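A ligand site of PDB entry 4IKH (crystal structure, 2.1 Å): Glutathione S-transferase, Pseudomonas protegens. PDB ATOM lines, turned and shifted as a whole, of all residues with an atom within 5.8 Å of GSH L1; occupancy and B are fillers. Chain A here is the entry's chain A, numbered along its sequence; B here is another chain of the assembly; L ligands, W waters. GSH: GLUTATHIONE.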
ATOM      1  N   THR A  30      17.648 -22.336 -13.036  1.00  0.00           N
ATOM      2  CA  THR A  30      16.835 -23.074 -13.993  1.00  0.00           C
ATOM      3  C   THR A  30      17.639 -24.293 -14.449  1.00  0.00           C
ATOM      4  O   THR A  30      18.825 -24.393 -14.143  1.00  0.00           O
ATOM      5  CB  THR A  30      16.528 -22.182 -15.197  1.00  0.00           C
ATOM      6  OG1 THR A  30      17.689 -22.092 -16.032  1.00  0.00           O
ATOM      7  CG2 THR A  30      16.118 -20.815 -14.725  1.00  0.00           C
ATOM      8  N   PRO A  31      16.997 -25.249 -15.159  1.00  0.00           N
ATOM      9  CA  PRO A  31      17.771 -26.418 -15.610  1.00  0.00           C
ATOM     10  C   PRO A  31      18.995 -26.025 -16.445  1.00  0.00           C
ATOM     11  O   PRO A  31      20.060 -26.585 -16.250  1.00  0.00           O
ATOM     12  CB  PRO A  31      16.792 -27.179 -16.504  1.00  0.00           C
ATOM     13  CG  PRO A  31      15.445 -26.719 -16.114  1.00  0.00           C
ATOM     14  CD  PRO A  31      15.577 -25.337 -15.562  1.00  0.00           C
ATOM     15  N   ASN A  32      18.850 -25.065 -17.354  1.00  0.00           N
ATOM     16  CA  ASN A  32      19.992 -24.635 -18.160  1.00  0.00           C
ATOM     17  C   ASN A  32      21.025 -23.852 -17.365  1.00  0.00           C
ATOM     18  O   ASN A  32      22.226 -23.963 -17.618  1.00  0.00           O
ATOM     19  CB  ASN A  32      19.541 -23.851 -19.392  1.00  0.00           C
ATOM     20  CG  ASN A  32      18.769 -24.706 -20.374  1.00  0.00           C
ATOM     21  OD1 ASN A  32      19.192 -25.809 -20.720  1.00  0.00           O
ATOM     22  ND2 ASN A  32      17.633 -24.195 -20.827  1.00  0.00           N
ATOM     23  N   GLY A  33      20.566 -23.073 -16.392  1.00  0.00           N
ATOM     24  CA  GLY A  33      21.475 -22.316 -15.548  1.00  0.00           C
ATOM     25  C   GLY A  33      22.296 -23.171 -14.603  1.00  0.00           C
ATOM     26  O   GLY A  33      23.519 -23.021 -14.499  1.00  0.00           O
ATOM     27  N   LYS A  35      23.253 -26.024 -14.975  1.00  0.00           N
ATOM     28  CA  LYS A  35      24.269 -26.782 -15.710  1.00  0.00           C
ATOM     29  C   LYS A  35      25.647 -26.166 -15.474  1.00  0.00           C
ATOM     30  O   LYS A  35      26.621 -26.874 -15.204  1.00  0.00           O
ATOM     31  CB  LYS A  35      23.991 -26.763 -17.223  1.00  0.00           C
ATOM     32  CG  LYS A  35      22.792 -27.575 -17.727  1.00  0.00           C
ATOM     33  CD  LYS A  35      22.729 -27.410 -19.280  1.00  0.00           C
ATOM     34  CE  LYS A  35      21.481 -28.012 -19.906  1.00  0.00           C
ATOM     35  NZ  LYS A  35      21.339 -27.569 -21.341  1.00  0.00           N
ATOM     36  N   PHE A  54      13.836 -12.769 -14.023  1.00  0.00           N
ATOM     37  CA  PHE A  54      12.895 -12.716 -15.138  1.00  0.00           C
ATOM     38  C   PHE A  54      11.692 -11.863 -14.781  1.00  0.00           C
ATOM     39  O   PHE A  54      11.026 -11.318 -15.662  1.00  0.00           O
ATOM     40  CB  PHE A  54      12.418 -14.132 -15.486  1.00  0.00           C
ATOM     41  CG  PHE A  54      13.480 -15.014 -16.060  1.00  0.00           C
ATOM     42  CD1 PHE A  54      14.699 -14.482 -16.476  1.00  0.00           C
ATOM     43  CD2 PHE A  54      13.260 -16.379 -16.190  1.00  0.00           C
ATOM     44  CE1 PHE A  54      15.687 -15.307 -17.002  1.00  0.00           C
ATOM     45  CE2 PHE A  54      14.239 -17.208 -16.720  1.00  0.00           C
ATOM     46  CZ  PHE A  54      15.453 -16.669 -17.129  1.00  0.00           C
ATOM     47  N   GLN A  59      16.619 -10.065 -18.456  1.00  0.00           N
ATOM     48  CA  GLN A  59      17.225 -10.735 -19.605  1.00  0.00           C
ATOM     49  C   GLN A  59      16.935  -9.997 -20.911  1.00  0.00           C
ATOM     50  O   GLN A  59      17.401 -10.404 -21.974  1.00  0.00           O
ATOM     51  CB  GLN A  59      16.773 -12.198 -19.692  1.00  0.00           C
ATOM     52  CG  GLN A  59      15.397 -12.417 -20.339  1.00  0.00           C
ATOM     53  CD  GLN A  59      14.252 -12.301 -19.363  1.00  0.00           C
ATOM     54  OE1 GLN A  59      14.336 -11.578 -18.363  1.00  0.00           O
ATOM     55  NE2 GLN A  59      13.167 -13.009 -19.652  1.00  0.00           N
ATOM     56  N   MET A  60      16.169  -8.910 -20.824  1.00  0.00           N
ATOM     57  CA  MET A  60      15.787  -8.128 -21.998  1.00  0.00           C
ATOM     58  C   MET A  60      16.542  -6.801 -22.058  1.00  0.00           C
ATOM     59  O   MET A  60      16.512  -6.107 -23.070  1.00  0.00           O
ATOM     60  CB  MET A  60      14.276  -7.874 -22.004  1.00  0.00           C
ATOM     61  CG  MET A  60      13.449  -9.148 -22.009  1.00  0.00           C
ATOM     62  SD  MET A  60      13.668 -10.165 -23.663  1.00  0.00           S
ATOM     63  CE  MET A  60      12.778 -11.818 -23.122  1.00  0.00           C
ATOM     64  N   ASN A  70      20.604 -13.677 -27.374  1.00  0.00           N
ATOM     65  CA  ASN A  70      19.402 -14.512 -27.460  1.00  0.00           C
ATOM     66  C   ASN A  70      18.437 -14.245 -26.302  1.00  0.00           C
ATOM     67  O   ASN A  70      17.421 -14.923 -26.174  1.00  0.00           O
ATOM     68  CB  ASN A  70      19.783 -16.003 -27.473  1.00  0.00           C
ATOM     69  CG  ASN A  70      18.627 -16.897 -27.900  1.00  0.00           C
ATOM     70  OD1 ASN A  70      17.793 -16.508 -28.707  1.00  0.00           O
ATOM     71  ND2 ASN A  70      18.593 -18.116 -27.358  1.00  0.00           N
ATOM     72  N   ASN A  71      18.781 -13.258 -25.475  1.00  0.00           N
ATOM     73  CA  ASN A  71      18.002 -12.927 -24.273  1.00  0.00           C
ATOM     74  C   ASN A  71      17.743 -14.107 -23.325  1.00  0.00           C
ATOM     75  O   ASN A  71      16.717 -14.158 -22.662  1.00  0.00           O
ATOM     76  CB  ASN A  71      16.695 -12.165 -24.584  1.00  0.00           C
ATOM     77  CG  ASN A  71      15.631 -13.027 -25.263  1.00  0.00           C
ATOM     78  OD1 ASN A  71      14.955 -13.842 -24.619  1.00  0.00           O
ATOM     79  ND2 ASN A  71      15.464 -12.847 -26.575  1.00  0.00           N
ATOM     80  N   LYS A  72      18.672 -15.036 -23.252  1.00  0.00           N
ATOM     81  CA  LYS A  72      18.530 -16.172 -22.378  1.00  0.00           C
ATOM     82  C   LYS A  72      19.751 -16.507 -21.507  1.00  0.00           C
ATOM     83  O   LYS A  72      20.871 -16.409 -21.940  1.00  0.00           O
ATOM     84  CB  LYS A  72      18.150 -17.393 -23.194  1.00  0.00           C
ATOM     85  CG  LYS A  72      16.784 -17.366 -23.802  1.00  0.00           C
ATOM     86  CD  LYS A  72      16.517 -18.664 -24.490  1.00  0.00           C
ATOM     87  CE  LYS A  72      15.419 -18.554 -25.522  1.00  0.00           C
ATOM     88  NZ  LYS A  72      14.151 -18.941 -24.917  1.00  0.00           N
ATOM     89  N   ILE A  73      19.503 -16.947 -20.289  1.00  0.00           N
ATOM     90  CA  ILE A  73      20.560 -17.413 -19.402  1.00  0.00           C
ATOM     91  C   ILE A  73      20.758 -18.913 -19.656  1.00  0.00           C
ATOM     92  O   ILE A  73      19.847 -19.581 -20.156  1.00  0.00           O
ATOM     93  CB  ILE A  73      20.201 -17.141 -17.895  1.00  0.00           C
ATOM     94  CG1 ILE A  73      18.905 -17.856 -17.491  1.00  0.00           C
ATOM     95  CG2 ILE A  73      20.075 -15.655 -17.635  1.00  0.00           C
ATOM     96  CD1 ILE A  73      19.127 -19.208 -16.848  1.00  0.00           C
ATOM     97  N   PRO A  74      21.940 -19.458 -19.315  1.00  0.00           N
ATOM     98  CA  PRO A  74      23.100 -18.812 -18.708  1.00  0.00           C
ATOM     99  C   PRO A  74      23.993 -18.118 -19.723  1.00  0.00           C
ATOM    100  O   PRO A  74      23.961 -18.419 -20.915  1.00  0.00           O
ATOM    101  CB  PRO A  74      23.879 -20.002 -18.121  1.00  0.00           C
ATOM    102  CG  PRO A  74      23.579 -21.120 -19.055  1.00  0.00           C
ATOM    103  CD  PRO A  74      22.142 -20.917 -19.475  1.00  0.00           C
ATOM    104  N   PHE A  90      27.372 -17.295 -24.411  1.00  0.00           N
ATOM    105  CA  PHE A  90      26.057 -17.779 -24.025  1.00  0.00           C
ATOM    106  C   PHE A  90      25.910 -19.202 -24.561  1.00  0.00           C
ATOM    107  O   PHE A  90      26.833 -19.711 -25.206  1.00  0.00           O
ATOM    108  CB  PHE A  90      24.916 -16.843 -24.449  1.00  0.00           C
ATOM    109  CG  PHE A  90      24.646 -16.781 -25.935  1.00  0.00           C
ATOM    110  CD1 PHE A  90      25.436 -16.003 -26.769  1.00  0.00           C
ATOM    111  CD2 PHE A  90      23.555 -17.452 -26.492  1.00  0.00           C
ATOM    112  CE1 PHE A  90      25.168 -15.921 -28.140  1.00  0.00           C
ATOM    113  CE2 PHE A  90      23.287 -17.384 -27.848  1.00  0.00           C
ATOM    114  CZ  PHE A  90      24.098 -16.607 -28.681  1.00  0.00           C
ATOM    115  N   GLU A  91      24.773 -19.826 -24.266  1.00  0.00           N
ATOM    116  CA  GLU A  91      24.520 -21.254 -24.540  1.00  0.00           C
ATOM    117  C   GLU A  91      25.228 -22.160 -23.527  1.00  0.00           C
ATOM    118  O   GLU A  91      26.462 -22.206 -23.414  1.00  0.00           O
ATOM    119  CB  GLU A  91      24.839 -21.660 -25.997  1.00  0.00           C
ATOM    120  CG  GLU A  91      23.919 -20.988 -27.038  1.00  0.00           C
ATOM    121  CD  GLU A  91      22.498 -21.520 -26.993  1.00  0.00           C
ATOM    122  OE1 GLU A  91      22.285 -22.701 -26.606  1.00  0.00           O
ATOM    123  OE2 GLU A  91      21.578 -20.751 -27.339  1.00  0.00           O
ATOM    124  N   SER A  92      24.421 -22.876 -22.759  1.00  0.00           N
ATOM    125  CA  SER A  92      24.943 -23.707 -21.689  1.00  0.00           C
ATOM    126  C   SER A  92      25.947 -24.730 -22.221  1.00  0.00           C
ATOM    127  O   SER A  92      27.050 -24.889 -21.660  1.00  0.00           O
ATOM    128  CB  SER A  92      23.789 -24.402 -20.954  1.00  0.00           C
ATOM    129  OG  SER A  92      22.971 -25.155 -21.830  1.00  0.00           O
ATOM    130  N   GLY A  93      25.596 -25.397 -23.312  1.00  0.00           N
ATOM    131  CA  GLY A  93      26.450 -26.433 -23.881  1.00  0.00           C
ATOM    132  C   GLY A  93      27.812 -25.932 -24.316  1.00  0.00           C
ATOM    133  O   GLY A  93      28.819 -26.624 -24.139  1.00  0.00           O
ATOM    134  N   MET A 125      21.162 -31.011 -25.752  1.00  0.00           N
ATOM    135  CA  MET A 125      20.960 -29.665 -26.302  1.00  0.00           C
ATOM    136  C   MET A 125      19.834 -29.569 -27.308  1.00  0.00           C
ATOM    137  O   MET A 125      19.061 -28.603 -27.295  1.00  0.00           O
ATOM    138  CB  MET A 125      22.268 -29.165 -26.935  1.00  0.00           C
ATOM    139  CG  MET A 125      23.348 -28.802 -25.885  1.00  0.00           C
ATOM    140  SD  MET A 125      22.709 -27.355 -24.696  1.00  0.00           S
ATOM    141  CE  MET A 125      22.659 -25.898 -26.106  1.00  0.00           C
ATOM    142  N   TRP A 191      17.809 -31.310 -16.176  1.00  0.00           N
ATOM    143  CA  TRP A 191      16.550 -31.264 -16.923  1.00  0.00           C
ATOM    144  C   TRP A 191      15.580 -32.383 -16.518  1.00  0.00           C
ATOM    145  O   TRP A 191      14.372 -32.165 -16.427  1.00  0.00           O
ATOM    146  CB  TRP A 191      16.799 -31.332 -18.425  1.00  0.00           C
ATOM    147  CG  TRP A 191      16.819 -29.956 -19.069  1.00  0.00           C
ATOM    148  CD1 TRP A 191      17.917 -29.264 -19.522  1.00  0.00           C
ATOM    149  CD2 TRP A 191      15.687 -29.114 -19.293  1.00  0.00           C
ATOM    150  NE1 TRP A 191      17.532 -28.054 -20.034  1.00  0.00           N
ATOM    151  CE2 TRP A 191      16.173 -27.932 -19.906  1.00  0.00           C
ATOM    152  CE3 TRP A 191      14.323 -29.235 -19.049  1.00  0.00           C
ATOM    153  CZ2 TRP A 191      15.321 -26.883 -20.273  1.00  0.00           C
ATOM    154  CZ3 TRP A 191      13.484 -28.196 -19.412  1.00  0.00           C
ATOM    155  CH2 TRP A 191      13.987 -27.037 -20.018  1.00  0.00           C
ATOM    156  N   MET B 122      25.585 -24.003 -30.931  1.00  0.00           N
ATOM    157  CA  MET B 122      24.618 -24.390 -29.894  1.00  0.00           C
ATOM    158  C   MET B 122      23.306 -23.627 -30.054  1.00  0.00           C
ATOM    159  O   MET B 122      22.231 -24.200 -29.871  1.00  0.00           O
ATOM    160  CB  MET B 122      25.183 -24.159 -28.497  1.00  0.00           C
ATOM    161  CG  MET B 122      26.340 -25.057 -28.173  1.00  0.00           C
ATOM    162  SD  MET B 122      25.788 -26.939 -28.262  1.00  0.00           S
ATOM    163  CE  MET B 122      27.457 -27.625 -27.538  1.00  0.00           C
ATOM    164  N   GLY B 126      20.038 -25.918 -30.211  1.00  0.00           N
ATOM    165  CA  GLY B 126      19.023 -25.857 -29.170  1.00  0.00           C
ATOM    166  C   GLY B 126      17.888 -24.897 -29.461  1.00  0.00           C
ATOM    167  O   GLY B 126      16.904 -24.860 -28.727  1.00  0.00           O
ATOM    168  N   GLY B 127      18.010 -24.123 -30.525  1.00  0.00           N
ATOM    169  CA  GLY B 127      16.994 -23.115 -30.791  1.00  0.00           C
ATOM    170  C   GLY B 127      16.426 -23.219 -32.179  1.00  0.00           C
ATOM    171  O   GLY B 127      15.276 -23.586 -32.357  1.00  0.00           O
HETATM  172  N1  GSH L   1      19.921 -23.355 -25.562  1.00  0.00           N
HETATM  173  CA1 GSH L   1      19.999 -22.455 -24.477  1.00  0.00           C
HETATM  174  C1  GSH L   1      21.051 -22.890 -23.493  1.00  0.00           C
HETATM  175  O11 GSH L   1      21.281 -24.127 -23.333  1.00  0.00           O
HETATM  176  O12 GSH L   1      21.711 -22.043 -22.816  1.00  0.00           O
HETATM  177  CB1 GSH L   1      18.690 -22.397 -23.774  1.00  0.00           C
HETATM  178  CG1 GSH L   1      18.785 -21.361 -22.657  1.00  0.00           C
HETATM  179  CD1 GSH L   1      17.426 -21.090 -22.046  1.00  0.00           C
HETATM  180  OE1 GSH L   1      16.434 -21.608 -22.507  1.00  0.00           O
HETATM  181  N2  GSH L   1      17.319 -20.209 -20.884  1.00  0.00           N
HETATM  182  CA2 GSH L   1      16.038 -19.961 -20.303  1.00  0.00           C
HETATM  183  C2  GSH L   1      15.855 -18.454 -20.370  1.00  0.00           C
HETATM  184  O2  GSH L   1      16.831 -17.725 -20.194  1.00  0.00           O
HETATM  185  CB2 GSH L   1      16.006 -20.392 -18.869  1.00  0.00           C
HETATM  186  SG2 GSH L   1      16.340 -22.137 -18.684  1.00  0.00           S
HETATM  187  N3  GSH L   1      14.562 -17.856 -20.656  1.00  0.00           N
HETATM  188  CA3 GSH L   1      14.444 -16.406 -20.691  1.00  0.00           C
HETATM  189  C3  GSH L   1      13.580 -16.003 -21.829  1.00  0.00           C
HETATM  190  O31 GSH L   1      13.380 -16.795 -22.793  1.00  0.00           O
HETATM  191  O32 GSH L   1      13.034 -14.870 -21.821  1.00  0.00           O
HETATM  192  N1  GSH L   2       9.045 -17.860 -22.219  1.00  0.00           N
HETATM  193  CA1 GSH L   2       9.691 -18.620 -23.217  1.00  0.00           C
HETATM  194  C1  GSH L   2       8.832 -19.778 -23.637  1.00  0.00           C
HETATM  195  O11 GSH L   2       7.582 -19.752 -23.413  1.00  0.00           O
HETATM  196  O12 GSH L   2       9.355 -20.770 -24.215  1.00  0.00           O
HETATM  197  CB1 GSH L   2      10.977 -19.132 -22.658  1.00  0.00           C
HETATM  198  CG1 GSH L   2      10.749 -19.986 -21.402  1.00  0.00           C
HETATM  199  CD1 GSH L   2      12.011 -20.794 -21.247  1.00  0.00           C
HETATM  200  OE1 GSH L   2      13.066 -20.271 -21.560  1.00  0.00           O
HETATM  201  N2  GSH L   2      11.991 -22.179 -20.763  1.00  0.00           N
HETATM  202  CA2 GSH L   2      13.221 -22.912 -20.650  1.00  0.00           C
HETATM  203  C2  GSH L   2      13.378 -23.840 -21.839  1.00  0.00           C
HETATM  204  O2  GSH L   2      12.382 -24.414 -22.325  1.00  0.00           O
HETATM  205  CB2 GSH L   2      13.226 -23.722 -19.391  1.00  0.00           C
HETATM  206  SG2 GSH L   2      13.190 -22.686 -17.953  1.00  0.00           S
HETATM  207  N3  GSH L   2      14.671 -24.096 -22.469  1.00  0.00           N
HETATM  208  CA3 GSH L   2      14.736 -25.003 -23.618  1.00  0.00           C
HETATM  209  C3  GSH L   2      16.117 -25.574 -23.822  1.00  0.00           C
HETATM  210  O31 GSH L   2      16.948 -25.622 -22.888  1.00  0.00           O
HETATM  211  O32 GSH L   2      16.446 -26.015 -24.941  1.00  0.00           O
HETATM  212  O   HOH W   1      22.345 -19.432 -23.121  1.00  0.00           O
HETATM  213  O   HOH W   2      19.063 -26.460 -25.722  1.00  0.00           O
HETATM  214  O   HOH W   3      15.455 -21.992 -24.819  1.00  0.00           O
HETATM  215  O   HOH W   4      12.629 -15.834 -25.255  1.00  0.00           O
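A nitrogen (N3) of GSH L1 is in hydrogen-bond range of an oxygen (OE1) of GSH L2 (3.0 Å).
Water W3 lies within hydrogen-bond range of an oxygen (OE1) of GSH L1 (2.5 Å), a nitrogen (N3) of GSH L2 (3.3 Å) and the side-chain amino group (NZ) of Lys 72 (3.3 Å). Water W1 lies within hydrogen-bond range of an oxygen (O12) of GSH L1, the backbone NH of Glu 91 and the backbone carbonyl oxygen of Pro 74. Water W4 lies within hydrogen-bond range of an oxygen (O31) of GSH L1, the side-chain amide oxygen of Asn 71 and the side-chain amino group of Lys 72. Water W2 lies within hydrogen-bond range of O of Met 125 (2.7 Å), O32 of GSH L2 (2.8 Å) and N1 of GSH L1 (3.2 Å).
A nitrogen (N2) of GSH L1 lies within hydrogen-bond range of the backbone carbonyl oxygen (O) of Ile 73. The side-chain amide nitrogen (ND2) of Asn 32 lies close to a sulfur (SG2) of GSH L1. OG of Ser 92 sits at hydrogen-bond distance from O11 of GSH L1. NZ of Lys 35 lies within salt-bridge range of O11 of GSH L1, 3.98 Å away. N of Ser 92 is in hydrogen-bond range of O12 of GSH L1 (2.8 Å). An oxygen (O2) of GSH L1 is in hydrogen-bond range of the backbone NH (N) of Ile 73. SG2 of GSH L1 sits close to OG1 of Thr 30. O31 of GSH L2 is in hydrogen-bond range of ND2 of Asn 32 (2.6 Å). The side-chain amino group of Lys 72 is in salt-bridge range of an oxygen (O31) of GSH L1 (3.1 Å). The side-chain amide nitrogen of Gln 59 lies within hydrogen-bond range of an oxygen (O32) of GSH L1, 2.9 Å away. N1 of GSH L1 is in salt-bridge range of OE1 of Glu 91.
The side-chain sulfur of Met 125 lies close to an oxygen (O11) of GSH L1. Phe 54 touches GSH L1. CE of Met 60 touches O32 of GSH L1, at 3.3 Å. Asn 71 touches GSH L1. Pro 74 touches GSH L1 (CD to O12, 3.6 Å). Of the 22 residues printed, 13 come within 4 Å of GSH L1. Along chain A the residues within 4 Å of GSH L1 span positions 30 to 125.
The indole nitrogen of Trp 191 lies within hydrogen-bond range of the side-chain amide oxygen of Asn 32, 2.9 Å away. The backbone NH (N) of Asn 32 lies close to the side-chain hydroxyl (OG1) of Thr 30 (3.5 Å). The side-chain amino group of Lys 35 lies within hydrogen-bond range of the side-chain sulfur of Met 125, at 3.6 Å. N of Gly 33 is in hydrogen-bond range of OG1 of Thr 30, at 3.1 Å. The backbone NH of Gly 93 lies within hydrogen-bond range of the side-chain sulfur of Met 125, at 3.8 Å. The side-chain amide oxygen (OD1) of Asn 32 is in hydrogen-bond range of the side-chain amino group (NZ) of Lys 35 (2.8 Å). OG of Ser 92 lies within hydrogen-bond range of NZ of Lys 35, 3.0 Å away. The side-chain sulfur (SD) of Met 125 is in hydrogen-bond range of the side-chain hydroxyl (OG) of Ser 92 (3.6 Å).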
